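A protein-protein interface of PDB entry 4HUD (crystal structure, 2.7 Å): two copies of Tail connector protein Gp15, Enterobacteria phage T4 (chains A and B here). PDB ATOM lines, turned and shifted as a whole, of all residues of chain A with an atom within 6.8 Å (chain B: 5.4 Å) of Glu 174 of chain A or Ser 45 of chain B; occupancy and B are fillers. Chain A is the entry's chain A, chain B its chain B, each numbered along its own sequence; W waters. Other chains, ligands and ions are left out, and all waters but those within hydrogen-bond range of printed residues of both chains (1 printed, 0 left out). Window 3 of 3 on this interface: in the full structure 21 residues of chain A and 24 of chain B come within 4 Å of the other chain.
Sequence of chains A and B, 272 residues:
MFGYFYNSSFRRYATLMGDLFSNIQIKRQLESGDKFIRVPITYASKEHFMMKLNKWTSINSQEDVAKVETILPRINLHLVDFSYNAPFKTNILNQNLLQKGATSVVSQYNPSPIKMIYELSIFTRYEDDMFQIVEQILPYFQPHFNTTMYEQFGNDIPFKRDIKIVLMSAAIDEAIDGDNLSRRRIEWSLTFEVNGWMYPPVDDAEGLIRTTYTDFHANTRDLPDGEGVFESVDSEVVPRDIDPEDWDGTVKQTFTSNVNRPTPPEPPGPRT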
ATOM      1  N   GLU A 127     -23.875  -1.431  -6.230  1.00  0.00           N
ATOM      2  CA  GLU A 127     -24.725  -2.110  -5.261  1.00  0.00           C
ATOM      3  C   GLU A 127     -24.529  -1.594  -3.826  1.00  0.00           C
ATOM      4  O   GLU A 127     -25.491  -1.452  -3.074  1.00  0.00           O
ATOM      5  CB  GLU A 127     -24.435  -3.614  -5.322  1.00  0.00           C
ATOM      6  CG  GLU A 127     -25.433  -4.461  -4.597  1.00  0.00           C
ATOM      7  CD  GLU A 127     -25.832  -5.680  -5.391  1.00  0.00           C
ATOM      8  OE1 GLU A 127     -27.010  -5.754  -5.883  1.00  0.00           O
ATOM      9  OE2 GLU A 127     -24.941  -6.552  -5.529  1.00  0.00           O
ATOM     10  N   ILE A 172     -37.081  -3.194  -8.040  1.00  0.00           N
ATOM     11  CA  ILE A 172     -35.654  -3.303  -8.362  1.00  0.00           C
ATOM     12  C   ILE A 172     -35.379  -3.551  -9.857  1.00  0.00           C
ATOM     13  O   ILE A 172     -35.994  -4.426 -10.463  1.00  0.00           O
ATOM     14  CB  ILE A 172     -35.024  -4.413  -7.506  1.00  0.00           C
ATOM     15  CG1 ILE A 172     -35.109  -4.029  -6.026  1.00  0.00           C
ATOM     16  CG2 ILE A 172     -33.584  -4.683  -7.920  1.00  0.00           C
ATOM     17  CD1 ILE A 172     -34.606  -5.101  -5.072  1.00  0.00           C
ATOM     18  N   ASP A 173     -34.461  -2.785 -10.445  1.00  0.00           N
ATOM     19  CA  ASP A 173     -34.132  -2.914 -11.873  1.00  0.00           C
ATOM     20  C   ASP A 173     -32.701  -2.493 -12.258  1.00  0.00           C
ATOM     21  O   ASP A 173     -31.995  -1.832 -11.483  1.00  0.00           O
ATOM     22  CB  ASP A 173     -35.102  -2.092 -12.703  1.00  0.00           C
ATOM     23  CG  ASP A 173     -35.245  -2.623 -14.113  1.00  0.00           C
ATOM     24  OD1 ASP A 173     -34.896  -3.819 -14.332  1.00  0.00           O
ATOM     25  OD2 ASP A 173     -35.738  -1.856 -14.984  1.00  0.00           O
ATOM     26  N   GLU A 174     -32.285  -2.847 -13.473  1.00  0.00           N
ATOM     27  CA  GLU A 174     -31.006  -2.368 -13.984  1.00  0.00           C
ATOM     28  C   GLU A 174     -31.102  -1.610 -15.315  1.00  0.00           C
ATOM     29  O   GLU A 174     -32.197  -1.239 -15.754  1.00  0.00           O
ATOM     30  CB  GLU A 174     -30.021  -3.517 -14.103  1.00  0.00           C
ATOM     31  CG  GLU A 174     -29.346  -3.846 -12.787  1.00  0.00           C
ATOM     32  CD  GLU A 174     -28.080  -4.637 -12.981  1.00  0.00           C
ATOM     33  OE1 GLU A 174     -27.906  -5.189 -14.086  1.00  0.00           O
ATOM     34  OE2 GLU A 174     -27.267  -4.713 -12.035  1.00  0.00           O
ATOM     35  N   ALA A 175     -29.938  -1.383 -15.929  1.00  0.00           N
ATOM     36  CA  ALA A 175     -29.800  -0.755 -17.250  1.00  0.00           C
ATOM     37  C   ALA A 175     -28.324  -0.787 -17.648  1.00  0.00           C
ATOM     38  O   ALA A 175     -27.569   0.135 -17.344  1.00  0.00           O
ATOM     39  CB  ALA A 175     -30.306   0.677 -17.231  1.00  0.00           C
ATOM     40  N   ILE A 176     -27.930  -1.835 -18.361  1.00  0.00           N
ATOM     41  CA  ILE A 176     -26.522  -2.196 -18.508  1.00  0.00           C
ATOM     42  C   ILE A 176     -25.850  -1.639 -19.773  1.00  0.00           C
ATOM     43  O   ILE A 176     -26.527  -1.135 -20.677  1.00  0.00           O
ATOM     44  CB  ILE A 176     -26.362  -3.742 -18.460  1.00  0.00           C
ATOM     45  CG1 ILE A 176     -27.465  -4.362 -17.592  1.00  0.00           C
ATOM     46  CG2 ILE A 176     -24.972  -4.158 -17.959  1.00  0.00           C
ATOM     47  CD1 ILE A 176     -27.396  -5.875 -17.478  1.00  0.00           C
ATOM     48  N   ARG A 183     -21.191  -0.629 -17.006  1.00  0.00           N
ATOM     49  CA  ARG A 183     -21.469  -1.509 -15.870  1.00  0.00           C
ATOM     50  C   ARG A 183     -22.926  -2.008 -15.690  1.00  0.00           C
ATOM     51  O   ARG A 183     -23.126  -3.219 -15.575  1.00  0.00           O
ATOM     52  CB  ARG A 183     -20.901  -0.926 -14.560  1.00  0.00           C
ATOM     53  N   ARG A 184     -23.942  -1.134 -15.655  1.00  0.00           N
ATOM     54  CA  ARG A 184     -23.833   0.322 -15.769  1.00  0.00           C
ATOM     55  C   ARG A 184     -24.556   1.084 -14.668  1.00  0.00           C
ATOM     56  O   ARG A 184     -23.958   1.914 -13.988  1.00  0.00           O
ATOM     57  CB  ARG A 184     -24.330   0.809 -17.132  1.00  0.00           C
ATOM     58  CG  ARG A 184     -23.367   1.742 -17.849  1.00  0.00           C
ATOM     59  CD  ARG A 184     -24.117   2.756 -18.692  1.00  0.00           C
ATOM     60  NE  ARG A 184     -25.298   2.163 -19.307  1.00  0.00           N
ATOM     61  CZ  ARG A 184     -26.544   2.507 -19.004  1.00  0.00           C
ATOM     62  NH1 ARG A 184     -26.771   3.440 -18.086  1.00  0.00           N
ATOM     63  NH2 ARG A 184     -27.564   1.913 -19.610  1.00  0.00           N
ATOM     64  N   ARG A 185     -25.846   0.815 -14.501  1.00  0.00           N
ATOM     65  CA  ARG A 185     -26.670   1.658 -13.635  1.00  0.00           C
ATOM     66  C   ARG A 185     -27.809   0.945 -12.886  1.00  0.00           C
ATOM     67  O   ARG A 185     -28.727   0.409 -13.509  1.00  0.00           O
ATOM     68  CB  ARG A 185     -27.236   2.816 -14.472  1.00  0.00           C
ATOM     69  CG  ARG A 185     -28.009   3.813 -13.673  1.00  0.00           C
ATOM     70  CD  ARG A 185     -28.371   5.068 -14.481  1.00  0.00           C
ATOM     71  NE  ARG A 185     -29.526   4.968 -15.370  1.00  0.00           N
ATOM     72  CZ  ARG A 185     -29.622   5.619 -16.528  1.00  0.00           C
ATOM     73  NH1 ARG A 185     -28.635   6.396 -16.942  1.00  0.00           N
ATOM     74  NH2 ARG A 185     -30.705   5.493 -17.281  1.00  0.00           N
ATOM     75  N   ILE A 186     -27.785   0.999 -11.553  1.00  0.00           N
ATOM     76  CA  ILE A 186     -28.814   0.341 -10.732  1.00  0.00           C
ATOM     77  C   ILE A 186     -29.950   1.306 -10.419  1.00  0.00           C
ATOM     78  O   ILE A 186     -29.691   2.458 -10.070  1.00  0.00           O
ATOM     79  CB  ILE A 186     -28.248  -0.158  -9.372  1.00  0.00           C
ATOM     80  CG1 ILE A 186     -27.189  -1.246  -9.571  1.00  0.00           C
ATOM     81  CG2 ILE A 186     -29.354  -0.719  -8.494  1.00  0.00           C
ATOM     82  CD1 ILE A 186     -25.787  -0.754  -9.748  1.00  0.00           C
ATOM     83  N   GLU A 187     -31.196   0.841 -10.538  1.00  0.00           N
ATOM     84  CA  GLU A 187     -32.368   1.669 -10.224  1.00  0.00           C
ATOM     85  C   GLU A 187     -33.364   0.946  -9.311  1.00  0.00           C
ATOM     86  O   GLU A 187     -33.985  -0.041  -9.708  1.00  0.00           O
ATOM     87  CB  GLU A 187     -33.120   2.106 -11.487  1.00  0.00           C
ATOM     88  CG  GLU A 187     -34.387   2.880 -11.141  1.00  0.00           C
ATOM     89  CD  GLU A 187     -35.532   2.705 -12.149  1.00  0.00           C
ATOM     90  OE1 GLU A 187     -36.702   2.797 -11.714  1.00  0.00           O
ATOM     91  OE2 GLU A 187     -35.282   2.481 -13.359  1.00  0.00           O
ATOM     92  N   TYR B  43     -23.310 -13.435  -7.017  1.00  0.00           N
ATOM     93  CA  TYR B  43     -24.375 -12.508  -6.660  1.00  0.00           C
ATOM     94  C   TYR B  43     -24.445 -11.393  -7.687  1.00  0.00           C
ATOM     95  O   TYR B  43     -23.528 -10.615  -7.821  1.00  0.00           O
ATOM     96  CB  TYR B  43     -24.139 -11.977  -5.261  1.00  0.00           C
ATOM     97  CG  TYR B  43     -25.282 -11.205  -4.673  1.00  0.00           C
ATOM     98  CD1 TYR B  43     -26.333 -11.850  -4.049  1.00  0.00           C
ATOM     99  CD2 TYR B  43     -25.286  -9.819  -4.699  1.00  0.00           C
ATOM    100  CE1 TYR B  43     -27.368 -11.140  -3.483  1.00  0.00           C
ATOM    101  CE2 TYR B  43     -26.318  -9.102  -4.146  1.00  0.00           C
ATOM    102  CZ  TYR B  43     -27.360  -9.761  -3.539  1.00  0.00           C
ATOM    103  OH  TYR B  43     -28.387  -9.024  -2.989  1.00  0.00           O
ATOM    104  N   ALA B  44     -25.516 -11.364  -8.457  1.00  0.00           N
ATOM    105  CA  ALA B  44     -25.605 -10.455  -9.584  1.00  0.00           C
ATOM    106  C   ALA B  44     -27.023 -10.341 -10.108  1.00  0.00           C
ATOM    107  O   ALA B  44     -27.830 -11.240  -9.950  1.00  0.00           O
ATOM    108  CB  ALA B  44     -24.676 -10.896 -10.695  1.00  0.00           C
ATOM    109  N   SER B  45     -27.326  -9.212 -10.726  1.00  0.00           N
ATOM    110  CA  SER B  45     -28.592  -9.089 -11.407  1.00  0.00           C
ATOM    111  C   SER B  45     -28.588 -10.199 -12.436  1.00  0.00           C
ATOM    112  O   SER B  45     -27.550 -10.483 -13.028  1.00  0.00           O
ATOM    113  CB  SER B  45     -28.743  -7.718 -12.060  1.00  0.00           C
ATOM    114  OG  SER B  45     -28.614  -7.816 -13.468  1.00  0.00           O
ATOM    115  N   LYS B  46     -29.741 -10.823 -12.640  1.00  0.00           N
ATOM    116  CA  LYS B  46     -29.803 -12.005 -13.475  1.00  0.00           C
ATOM    117  C   LYS B  46     -29.394 -11.698 -14.912  1.00  0.00           C
ATOM    118  O   LYS B  46     -28.604 -12.421 -15.499  1.00  0.00           O
ATOM    119  CB  LYS B  46     -31.187 -12.645 -13.398  1.00  0.00           C
ATOM    120  CG  LYS B  46     -31.261 -14.049 -13.984  1.00  0.00           C
ATOM    121  CD  LYS B  46     -32.602 -14.661 -13.637  1.00  0.00           C
ATOM    122  CE  LYS B  46     -32.788 -16.062 -14.174  1.00  0.00           C
ATOM    123  NZ  LYS B  46     -34.185 -16.476 -13.874  1.00  0.00           N
ATOM    124  N   GLU B  47     -29.913 -10.613 -15.465  1.00  0.00           N
ATOM    125  CA  GLU B  47     -29.590 -10.219 -16.832  1.00  0.00           C
ATOM    126  C   GLU B  47     -28.082 -10.129 -17.017  1.00  0.00           C
ATOM    127  O   GLU B  47     -27.529 -10.655 -17.982  1.00  0.00           O
ATOM    128  CB  GLU B  47     -30.247  -8.885 -17.181  1.00  0.00           C
ATOM    129  CG  GLU B  47     -30.745  -8.830 -18.605  1.00  0.00           C
ATOM    130  CD  GLU B  47     -31.703  -9.968 -18.935  1.00  0.00           C
ATOM    131  OE1 GLU B  47     -32.921  -9.810 -18.670  1.00  0.00           O
ATOM    132  OE2 GLU B  47     -31.240 -11.018 -19.444  1.00  0.00           O
ATOM    133  N   HIS B  48     -27.440  -9.441 -16.078  1.00  0.00           N
ATOM    134  CA  HIS B  48     -25.994  -9.283 -16.008  1.00  0.00           C
ATOM    135  C   HIS B  48     -25.289 -10.628 -16.062  1.00  0.00           C
ATOM    136  O   HIS B  48     -24.425 -10.875 -16.924  1.00  0.00           O
ATOM    137  CB  HIS B  48     -25.650  -8.602 -14.684  1.00  0.00           C
ATOM    138  CG  HIS B  48     -24.205  -8.257 -14.521  1.00  0.00           C
ATOM    139  ND1 HIS B  48     -23.646  -7.950 -13.298  1.00  0.00           N
ATOM    140  CD2 HIS B  48     -23.200  -8.145 -15.429  1.00  0.00           C
ATOM    141  CE1 HIS B  48     -22.364  -7.669 -13.452  1.00  0.00           C
ATOM    142  NE2 HIS B  48     -22.072  -7.785 -14.740  1.00  0.00           N
ATOM    143  N   PHE B  49     -25.652 -11.490 -15.117  1.00  0.00           N
ATOM    144  CA  PHE B  49     -25.048 -12.807 -15.014  1.00  0.00           C
ATOM    145  C   PHE B  49     -25.161 -13.545 -16.335  1.00  0.00           C
ATOM    146  O   PHE B  49     -24.197 -14.125 -16.802  1.00  0.00           O
ATOM    147  CB  PHE B  49     -25.692 -13.619 -13.895  1.00  0.00           C
ATOM    148  CG  PHE B  49     -25.194 -15.025 -13.825  1.00  0.00           C
ATOM    149  CD1 PHE B  49     -23.980 -15.314 -13.220  1.00  0.00           C
ATOM    150  CD2 PHE B  49     -25.926 -16.060 -14.374  1.00  0.00           C
ATOM    151  CE1 PHE B  49     -23.515 -16.600 -13.160  1.00  0.00           C
ATOM    152  CE2 PHE B  49     -25.468 -17.342 -14.318  1.00  0.00           C
ATOM    153  CZ  PHE B  49     -24.263 -17.622 -13.709  1.00  0.00           C
ATOM    154  N   MET B  50     -26.322 -13.478 -16.963  1.00  0.00           N
ATOM    155  CA  MET B  50     -26.525 -14.209 -18.204  1.00  0.00           C
ATOM    156  C   MET B  50     -25.694 -13.619 -19.340  1.00  0.00           C
ATOM    157  O   MET B  50     -25.197 -14.355 -20.188  1.00  0.00           O
ATOM    158  CB  MET B  50     -28.009 -14.280 -18.567  1.00  0.00           C
ATOM    159  CG  MET B  50     -28.584 -15.674 -18.409  1.00  0.00           C
ATOM    160  SD  MET B  50     -30.295 -15.698 -17.842  1.00  0.00           S
ATOM    161  CE  MET B  50     -31.136 -14.933 -19.233  1.00  0.00           C
ATOM    162  N   ASN B  76     -26.351 -18.519  -9.691  1.00  0.00           N
ATOM    163  CA  ASN B  76     -26.324 -17.084  -9.529  1.00  0.00           C
ATOM    164  C   ASN B  76     -27.381 -16.722  -8.513  1.00  0.00           C
ATOM    165  O   ASN B  76     -28.488 -17.227  -8.582  1.00  0.00           O
ATOM    166  CB  ASN B  76     -26.618 -16.382 -10.840  1.00  0.00           C
ATOM    167  CG  ASN B  76     -26.457 -14.881 -10.722  1.00  0.00           C
ATOM    168  OD1 ASN B  76     -25.351 -14.386 -10.623  1.00  0.00           O
ATOM    169  ND2 ASN B  76     -27.562 -14.164 -10.662  1.00  0.00           N
ATOM    170  N   HIS B  78     -29.580 -13.540  -6.491  1.00  0.00           N
ATOM    171  CA  HIS B  78     -29.869 -12.087  -6.402  1.00  0.00           C
ATOM    172  C   HIS B  78     -31.123 -11.694  -5.643  1.00  0.00           C
ATOM    173  O   HIS B  78     -32.104 -12.425  -5.642  1.00  0.00           O
ATOM    174  CB  HIS B  78     -29.899 -11.410  -7.771  1.00  0.00           C
ATOM    175  CG  HIS B  78     -29.266 -10.051  -7.770  1.00  0.00           C
ATOM    176  ND1 HIS B  78     -29.810  -8.976  -8.443  1.00  0.00           N
ATOM    177  CD2 HIS B  78     -28.140  -9.599  -7.181  1.00  0.00           C
ATOM    178  CE1 HIS B  78     -29.037  -7.914  -8.270  1.00  0.00           C
ATOM    179  NE2 HIS B  78     -28.014  -8.269  -7.509  1.00  0.00           N
HETATM  180  O   HOH W   1     -25.452  -7.150 -11.454  1.00  0.00           O
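The side-chain hydroxyl of Ser 45 of chain B is in hydrogen-bond range of the backbone NH of His 48 of chain B, at 3.3 Å. O of Ile 176 of chain A lies within hydrogen-bond range of NH2 of Arg 184 of chain A, 3.4 Å away. The backbone carbonyl oxygen (O) of Ala 44 of chain B lies close to a ring nitrogen (ND1) of His 78 of chain B (3.4 Å). The backbone NH (N) of Ser 45 of chain B sits close to a ring nitrogen (ND1) of His 78 of chain B, 3.4 Å away.
Of the printed residues of chain B, Glu 127 of chain A touches Tyr 43 (3.2 Å) and His 78 (3.2 Å). Glu 174 of chain A touches just one residue of chain B: Ser 45. Of the printed residues of chain A, Ser 45 of chain B touches Glu 174. Printed residues of chain A within 4 Å of His 48 of chain B: Ile 176 (3.8 Å). Met 50 of chain B touches none of the printed residues of chain A. Asn 76 of chain B touches none of the printed residues of chain A. Of the printed residues of chain A, His 78 of chain B touches Glu 127. The nearest residue of chain B that does not touch Glu 174 of chain A is His 48 of chain B (4.1 Å). The nearest residue of chain A that does not touch Ser 45 of chain B is Ile 176 of chain A (4.6 Å). The nearest printed residue of chain B that does not touch Ile 176 of chain A is Glu 47 of chain B (4.2 Å).
No position is printed for both chains.
Among the printed residues, pairs that only touch across the chains: Glu 127 of chain A with Tyr 43 of chain B and Ile 176 of chain A with His 48 of chain B.
Water W1 lies within hydrogen-bond range of a ring nitrogen (ND1) of His 48 of chain B, the backbone NH (N) of Ser 45 of chain B and the side-chain carboxylate (OE2) of Glu 174 of chain A.
Hydrophobic or aromatic side chains of chain A that line the printed part of chain B: Ile 176. Among the printed residues, no Asp or Glu carboxylate lies within 4 Å of a Lys or Arg side-chain nitrogen of the other chain.
OE1 of Glu 127 of chain A sits at hydrogen-bond distance from NE2 of His 78 of chain B (3.2 Å). OE1 of Glu 174 of chain A is in hydrogen-bond range of OG of Ser 45 of chain B (2.8 Å).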
